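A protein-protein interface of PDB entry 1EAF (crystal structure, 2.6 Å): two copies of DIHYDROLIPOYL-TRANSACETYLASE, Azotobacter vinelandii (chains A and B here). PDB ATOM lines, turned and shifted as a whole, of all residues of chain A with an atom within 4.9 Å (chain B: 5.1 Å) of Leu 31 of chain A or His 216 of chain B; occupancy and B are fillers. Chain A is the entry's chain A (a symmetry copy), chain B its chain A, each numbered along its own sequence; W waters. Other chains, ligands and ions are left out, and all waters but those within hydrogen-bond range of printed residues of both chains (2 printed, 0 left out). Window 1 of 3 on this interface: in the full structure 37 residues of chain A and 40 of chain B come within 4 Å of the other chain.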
ATOM      1  N   GLY A  27      25.008   5.308   2.560  1.00  0.00           N
ATOM      2  CA  GLY A  27      24.999   4.564   3.796  1.00  0.00           C
ATOM      3  C   GLY A  27      25.894   5.207   4.825  1.00  0.00           C
ATOM      4  O   GLY A  27      25.399   5.456   5.913  1.00  0.00           O
ATOM      5  N   ALA A  28      27.147   5.557   4.514  1.00  0.00           N
ATOM      6  CA  ALA A  28      28.079   6.131   5.456  1.00  0.00           C
ATOM      7  C   ALA A  28      27.494   7.387   6.064  1.00  0.00           C
ATOM      8  O   ALA A  28      27.459   7.552   7.296  1.00  0.00           O
ATOM      9  CB  ALA A  28      29.388   6.492   4.783  1.00  0.00           C
ATOM     10  N   THR A  29      26.921   8.221   5.195  1.00  0.00           N
ATOM     11  CA  THR A  29      26.267   9.448   5.612  1.00  0.00           C
ATOM     12  C   THR A  29      25.023   9.218   6.462  1.00  0.00           C
ATOM     13  O   THR A  29      24.916   9.886   7.498  1.00  0.00           O
ATOM     14  CB  THR A  29      25.961  10.260   4.312  1.00  0.00           C
ATOM     15  OG1 THR A  29      27.245  10.686   3.824  1.00  0.00           O
ATOM     16  CG2 THR A  29      25.006  11.441   4.521  1.00  0.00           C
ATOM     17  N   ASN A  30      24.111   8.304   6.139  1.00  0.00           N
ATOM     18  CA  ASN A  30      22.955   8.114   6.992  1.00  0.00           C
ATOM     19  C   ASN A  30      23.374   7.564   8.357  1.00  0.00           C
ATOM     20  O   ASN A  30      22.861   8.010   9.391  1.00  0.00           O
ATOM     21  CB  ASN A  30      21.954   7.128   6.412  1.00  0.00           C
ATOM     22  CG  ASN A  30      21.452   7.483   5.023  1.00  0.00           C
ATOM     23  OD1 ASN A  30      21.423   8.628   4.566  1.00  0.00           O
ATOM     24  ND2 ASN A  30      21.094   6.500   4.210  1.00  0.00           N
ATOM     25  N   LEU A  31      24.365   6.648   8.395  1.00  0.00           N
ATOM     26  CA  LEU A  31      24.829   6.042   9.639  1.00  0.00           C
ATOM     27  C   LEU A  31      25.456   7.064  10.542  1.00  0.00           C
ATOM     28  O   LEU A  31      25.204   7.131  11.741  1.00  0.00           O
ATOM     29  CB  LEU A  31      25.854   4.929   9.371  1.00  0.00           C
ATOM     30  CG  LEU A  31      25.262   3.674   8.749  1.00  0.00           C
ATOM     31  CD1 LEU A  31      26.392   2.814   8.241  1.00  0.00           C
ATOM     32  CD2 LEU A  31      24.406   2.936   9.748  1.00  0.00           C
ATOM     33  N   HIS A  32      26.274   7.912   9.964  1.00  0.00           N
ATOM     34  CA  HIS A  32      26.887   8.923  10.762  1.00  0.00           C
ATOM     35  C   HIS A  32      25.844   9.921  11.244  1.00  0.00           C
ATOM     36  O   HIS A  32      25.988  10.375  12.380  1.00  0.00           O
ATOM     37  CB  HIS A  32      27.959   9.626   9.980  1.00  0.00           C
ATOM     38  CG  HIS A  32      28.960  10.287  10.910  1.00  0.00           C
ATOM     39  ND1 HIS A  32      29.012  10.300  12.256  1.00  0.00           N
ATOM     40  CD2 HIS A  32      30.014  11.044  10.475  1.00  0.00           C
ATOM     41  CE1 HIS A  32      30.020  11.026  12.622  1.00  0.00           C
ATOM     42  NE2 HIS A  32      30.613  11.474  11.550  1.00  0.00           N
ATOM     43  N   ARG A  33      24.773  10.206  10.479  1.00  0.00           N
ATOM     44  CA  ARG A  33      23.700  11.115  10.883  1.00  0.00           C
ATOM     45  C   ARG A  33      22.912  10.523  12.066  1.00  0.00           C
ATOM     46  O   ARG A  33      22.701  11.196  13.099  1.00  0.00           O
ATOM     47  CB  ARG A  33      22.792  11.321   9.703  1.00  0.00           C
ATOM     48  CG  ARG A  33      22.255  12.719   9.684  1.00  0.00           C
ATOM     49  CD  ARG A  33      20.987  12.955   8.849  1.00  0.00           C
ATOM     50  NE  ARG A  33      20.591  11.929   7.877  1.00  0.00           N
ATOM     51  CZ  ARG A  33      20.879  12.047   6.564  1.00  0.00           C
ATOM     52  NH1 ARG A  33      21.548  13.112   6.064  1.00  0.00           N
ATOM     53  NH2 ARG A  33      20.524  11.042   5.758  1.00  0.00           N
ATOM     54  N   SER A  34      22.530   9.227  11.969  1.00  0.00           N
ATOM     55  CA  SER A  34      21.900   8.545  13.083  1.00  0.00           C
ATOM     56  C   SER A  34      22.753   8.522  14.320  1.00  0.00           C
ATOM     57  O   SER A  34      22.253   8.840  15.389  1.00  0.00           O
ATOM     58  CB  SER A  34      21.602   7.127  12.773  1.00  0.00           C
ATOM     59  OG  SER A  34      20.738   7.106  11.639  1.00  0.00           O
ATOM     60  N   TRP A  35      24.038   8.198  14.178  1.00  0.00           N
ATOM     61  CA  TRP A  35      24.961   8.101  15.290  1.00  0.00           C
ATOM     62  C   TRP A  35      25.014   9.366  16.147  1.00  0.00           C
ATOM     63  O   TRP A  35      25.012   9.328  17.384  1.00  0.00           O
ATOM     64  CB  TRP A  35      26.373   7.769  14.739  1.00  0.00           C
ATOM     65  CG  TRP A  35      27.447   7.597  15.808  1.00  0.00           C
ATOM     66  CD1 TRP A  35      28.466   8.502  15.941  1.00  0.00           C
ATOM     67  CD2 TRP A  35      27.528   6.571  16.733  1.00  0.00           C
ATOM     68  NE1 TRP A  35      29.188   8.054  16.954  1.00  0.00           N
ATOM     69  CE2 TRP A  35      28.676   6.918  17.444  1.00  0.00           C
ATOM     70  CE3 TRP A  35      26.822   5.416  17.043  1.00  0.00           C
ATOM     71  CZ2 TRP A  35      29.127   6.127  18.496  1.00  0.00           C
ATOM     72  CZ3 TRP A  35      27.277   4.630  18.088  1.00  0.00           C
ATOM     73  CH2 TRP A  35      28.420   4.976  18.806  1.00  0.00           C
ATOM     74  N   LEU A 119      24.734  -1.745   1.843  1.00  0.00           N
ATOM     75  CA  LEU A 119      23.600  -2.198   2.614  1.00  0.00           C
ATOM     76  C   LEU A 119      22.307  -1.626   2.061  1.00  0.00           C
ATOM     77  O   LEU A 119      22.230  -0.414   1.793  1.00  0.00           O
ATOM     78  CB  LEU A 119      23.778  -1.749   4.070  1.00  0.00           C
ATOM     79  CG  LEU A 119      22.658  -1.946   5.059  1.00  0.00           C
ATOM     80  CD1 LEU A 119      22.530  -3.412   5.375  1.00  0.00           C
ATOM     81  CD2 LEU A 119      22.937  -1.139   6.290  1.00  0.00           C
ATOM     82  N   ILE A 177      23.039   0.093  14.922  1.00  0.00           N
ATOM     83  CA  ILE A 177      22.678   1.503  14.913  1.00  0.00           C
ATOM     84  C   ILE A 177      21.228   1.684  14.478  1.00  0.00           C
ATOM     85  O   ILE A 177      20.752   1.038  13.566  1.00  0.00           O
ATOM     86  CB  ILE A 177      23.659   2.261  13.972  1.00  0.00           C
ATOM     87  CG1 ILE A 177      25.013   2.325  14.653  1.00  0.00           C
ATOM     88  CG2 ILE A 177      23.172   3.670  13.690  1.00  0.00           C
ATOM     89  CD1 ILE A 177      26.138   2.697  13.685  1.00  0.00           C
ATOM     90  N   PRO B  39      30.695   6.030  13.455  1.00  0.00           N
ATOM     91  CA  PRO B  39      29.516   5.276  13.869  1.00  0.00           C
ATOM     92  C   PRO B  39      29.962   3.849  14.239  1.00  0.00           C
ATOM     93  O   PRO B  39      30.315   3.056  13.360  1.00  0.00           O
ATOM     94  CB  PRO B  39      28.580   5.348  12.643  1.00  0.00           C
ATOM     95  CG  PRO B  39      29.323   6.110  11.548  1.00  0.00           C
ATOM     96  CD  PRO B  39      30.783   6.106  11.998  1.00  0.00           C
ATOM     97  N   VAL B  41      29.897  -0.025  15.866  1.00  0.00           N
ATOM     98  CA  VAL B  41      29.096  -1.171  16.269  1.00  0.00           C
ATOM     99  C   VAL B  41      30.043  -2.124  16.970  1.00  0.00           C
ATOM    100  O   VAL B  41      31.211  -2.145  16.605  1.00  0.00           O
ATOM    101  CB  VAL B  41      28.464  -1.884  15.081  1.00  0.00           C
ATOM    102  CG1 VAL B  41      27.638  -3.115  15.507  1.00  0.00           C
ATOM    103  CG2 VAL B  41      27.464  -0.918  14.459  1.00  0.00           C
ATOM    104  N   TYR B 214      33.778  -1.820  15.159  1.00  0.00           N
ATOM    105  CA  TYR B 214      34.151  -1.411  13.840  1.00  0.00           C
ATOM    106  C   TYR B 214      33.391  -0.161  13.431  1.00  0.00           C
ATOM    107  O   TYR B 214      32.328   0.201  13.964  1.00  0.00           O
ATOM    108  CB  TYR B 214      33.877  -2.552  12.861  1.00  0.00           C
ATOM    109  CG  TYR B 214      32.469  -3.097  12.903  1.00  0.00           C
ATOM    110  CD1 TYR B 214      32.064  -4.078  13.801  1.00  0.00           C
ATOM    111  CD2 TYR B 214      31.590  -2.582  11.983  1.00  0.00           C
ATOM    112  CE1 TYR B 214      30.761  -4.548  13.739  1.00  0.00           C
ATOM    113  CE2 TYR B 214      30.304  -3.049  11.914  1.00  0.00           C
ATOM    114  CZ  TYR B 214      29.900  -4.020  12.788  1.00  0.00           C
ATOM    115  OH  TYR B 214      28.596  -4.477  12.612  1.00  0.00           O
ATOM    116  N   ASP B 215      34.002   0.509  12.467  1.00  0.00           N
ATOM    117  CA  ASP B 215      33.458   1.686  11.825  1.00  0.00           C
ATOM    118  C   ASP B 215      32.463   1.208  10.769  1.00  0.00           C
ATOM    119  O   ASP B 215      32.878   0.767   9.684  1.00  0.00           O
ATOM    120  CB  ASP B 215      34.607   2.423  11.190  1.00  0.00           C
ATOM    121  CG  ASP B 215      34.230   3.724  10.517  1.00  0.00           C
ATOM    122  OD1 ASP B 215      33.066   3.982  10.246  1.00  0.00           O
ATOM    123  OD2 ASP B 215      35.159   4.489  10.271  1.00  0.00           O
ATOM    124  N   HIS B 216      31.168   1.409  11.027  1.00  0.00           N
ATOM    125  CA  HIS B 216      30.166   0.901  10.110  1.00  0.00           C
ATOM    126  C   HIS B 216      30.076   1.634   8.759  1.00  0.00           C
ATOM    127  O   HIS B 216      29.402   1.175   7.820  1.00  0.00           O
ATOM    128  CB  HIS B 216      28.808   0.918  10.823  1.00  0.00           C
ATOM    129  CG  HIS B 216      27.771   0.023  10.160  1.00  0.00           C
ATOM    130  ND1 HIS B 216      27.676  -0.464   8.920  1.00  0.00           N
ATOM    131  CD2 HIS B 216      26.656  -0.391  10.830  1.00  0.00           C
ATOM    132  CE1 HIS B 216      26.580  -1.131   8.807  1.00  0.00           C
ATOM    133  NE2 HIS B 216      25.965  -1.090   9.955  1.00  0.00           N
ATOM    134  N   ARG B 217      30.751   2.782   8.609  1.00  0.00           N
ATOM    135  CA  ARG B 217      30.834   3.468   7.321  1.00  0.00           C
ATOM    136  C   ARG B 217      31.637   2.593   6.362  1.00  0.00           C
ATOM    137  O   ARG B 217      31.374   2.599   5.175  1.00  0.00           O
ATOM    138  CB  ARG B 217      31.571   4.812   7.408  1.00  0.00           C
ATOM    139  CG  ARG B 217      30.863   5.813   8.328  1.00  0.00           C
ATOM    140  CD  ARG B 217      31.697   7.059   8.530  1.00  0.00           C
ATOM    141  NE  ARG B 217      32.965   6.742   9.145  1.00  0.00           N
ATOM    142  CZ  ARG B 217      33.936   7.641   9.284  1.00  0.00           C
ATOM    143  NH1 ARG B 217      33.772   8.883   8.854  1.00  0.00           N
ATOM    144  NH2 ARG B 217      35.096   7.351   9.853  1.00  0.00           N
ATOM    145  N   VAL B 218      32.629   1.841   6.821  1.00  0.00           N
ATOM    146  CA  VAL B 218      33.463   1.010   5.980  1.00  0.00           C
ATOM    147  C   VAL B 218      33.033  -0.433   6.126  1.00  0.00           C
ATOM    148  O   VAL B 218      33.154  -1.200   5.177  1.00  0.00           O
ATOM    149  CB  VAL B 218      34.944   1.180   6.424  1.00  0.00           C
ATOM    150  CG1 VAL B 218      35.875   0.317   5.600  1.00  0.00           C
ATOM    151  CG2 VAL B 218      35.339   2.645   6.282  1.00  0.00           C
ATOM    152  N   ILE B 219      32.598  -0.924   7.294  1.00  0.00           N
ATOM    153  CA  ILE B 219      32.319  -2.345   7.446  1.00  0.00           C
ATOM    154  C   ILE B 219      30.910  -2.546   7.860  1.00  0.00           C
ATOM    155  O   ILE B 219      30.450  -1.929   8.818  1.00  0.00           O
ATOM    156  CB  ILE B 219      33.316  -2.933   8.489  1.00  0.00           C
ATOM    157  CG1 ILE B 219      34.612  -3.183   7.707  1.00  0.00           C
ATOM    158  CG2 ILE B 219      32.883  -4.280   9.104  1.00  0.00           C
ATOM    159  CD1 ILE B 219      35.711  -2.744   8.601  1.00  0.00           C
ATOM    160  N   ASN B 220      30.236  -3.412   7.123  1.00  0.00           N
ATOM    161  CA  ASN B 220      28.861  -3.757   7.445  1.00  0.00           C
ATOM    162  C   ASN B 220      28.820  -4.945   8.371  1.00  0.00           C
ATOM    163  O   ASN B 220      29.821  -5.630   8.609  1.00  0.00           O
ATOM    164  CB  ASN B 220      28.083  -4.004   6.144  1.00  0.00           C
ATOM    165  CG  ASN B 220      27.806  -2.629   5.487  1.00  0.00           C
ATOM    166  OD1 ASN B 220      27.501  -1.615   6.146  1.00  0.00           O
ATOM    167  ND2 ASN B 220      27.940  -2.421   4.179  1.00  0.00           N
ATOM    168  N   GLY B 221      27.627  -5.172   8.864  1.00  0.00           N
ATOM    169  CA  GLY B 221      27.343  -6.194   9.840  1.00  0.00           C
ATOM    170  C   GLY B 221      27.814  -7.594   9.458  1.00  0.00           C
ATOM    171  O   GLY B 221      28.472  -8.232  10.301  1.00  0.00           O
HETATM  172  O   HOH W   1      28.825   2.996   4.491  1.00  0.00           O
HETATM  173  O   HOH W   2      24.108  -1.384  12.573  1.00  0.00           O
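Water W1 lies within hydrogen-bond range of O of Arg 217 of chain B (2.7 Å) and N of Ala 28 of chain A (3.1 Å).
Water W2 lies within hydrogen-bond range of N of Ile 177 of chain A and NE2 of His 216 of chain B.
No position is printed for both chains.
Of the 7 pairs that touch across the chains among the printed residues, none has its exchanged pair printed and touching as well.
Of the 10 printed residues of chain B, 4 touch a printed residue of chain A.
Printed residues of chain A that touch a printed residue of chain B: Ala 28, Leu 31, His 32, Trp 35 and Ile 177.
Among the printed residues, 7 pairs touch across the chains.
Printed residues of chain B within 4 Å of Ala 28 of chain A: Arg 217.
Of the printed residues of chain B, Leu 31 of chain A touches Pro 39 and His 216.
Ser 34 of chain A touches none of the printed residues of chain B.
Printed residues of chain B within 4 Å of Ile 177 of chain A: Pro 39 and Val 41.
Of the printed residues of chain A, Val 41 of chain B touches Ile 177.
Asp 215 of chain B touches none of the printed residues of chain A.
His 216 of chain B touches just one residue of chain A: Leu 31 (3.5 Å).
Of the printed residues of chain A, Arg 217 of chain B touches Ala 28.
The nearest residue of chain B that does not touch Leu 31 of chain A is Arg 217 of chain B (4.4 Å).
The nearest printed residue of chain A that does not touch Pro 39 of chain B is Ala 28 of chain A (4.9 Å).
Ala 28 of chain A touches Arg 217 of chain B (CB to CB, 3.8 Å).
Pro 39 of chain B touches Leu 31 of chain A.
Leu 31 of chain A touches His 216 of chain B.
His 32 of chain A touches Pro 39 of chain B (CA to CG, 3.8 Å).
Trp 35 of chain A touches Pro 39 of chain B.
Ile 177 of chain A touches Pro 39 of chain B.
CD1 of Ile 177 of chain A touches CG2 of Val 41 of chain B (3.9 Å).
The backbone NH of His 216 of chain B is in hydrogen-bond range of the backbone carbonyl oxygen of Pro 39 of chain B (3.0 Å).
N of Tyr 214 of chain B is in hydrogen-bond range of O of Val 41 of chain B, 3.0 Å away.
The side-chain carboxylate of Asp 215 of chain B is in salt-bridge range of the guanidinium group of Arg 217 of chain B, at 2.9 Å.
O of Ile 219 of chain B sits close to ND1 of His 216 of chain B (3.1 Å).
ND1 of His 216 of chain B sits close to OD1 of Asn 220 of chain B (3.0 Å).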
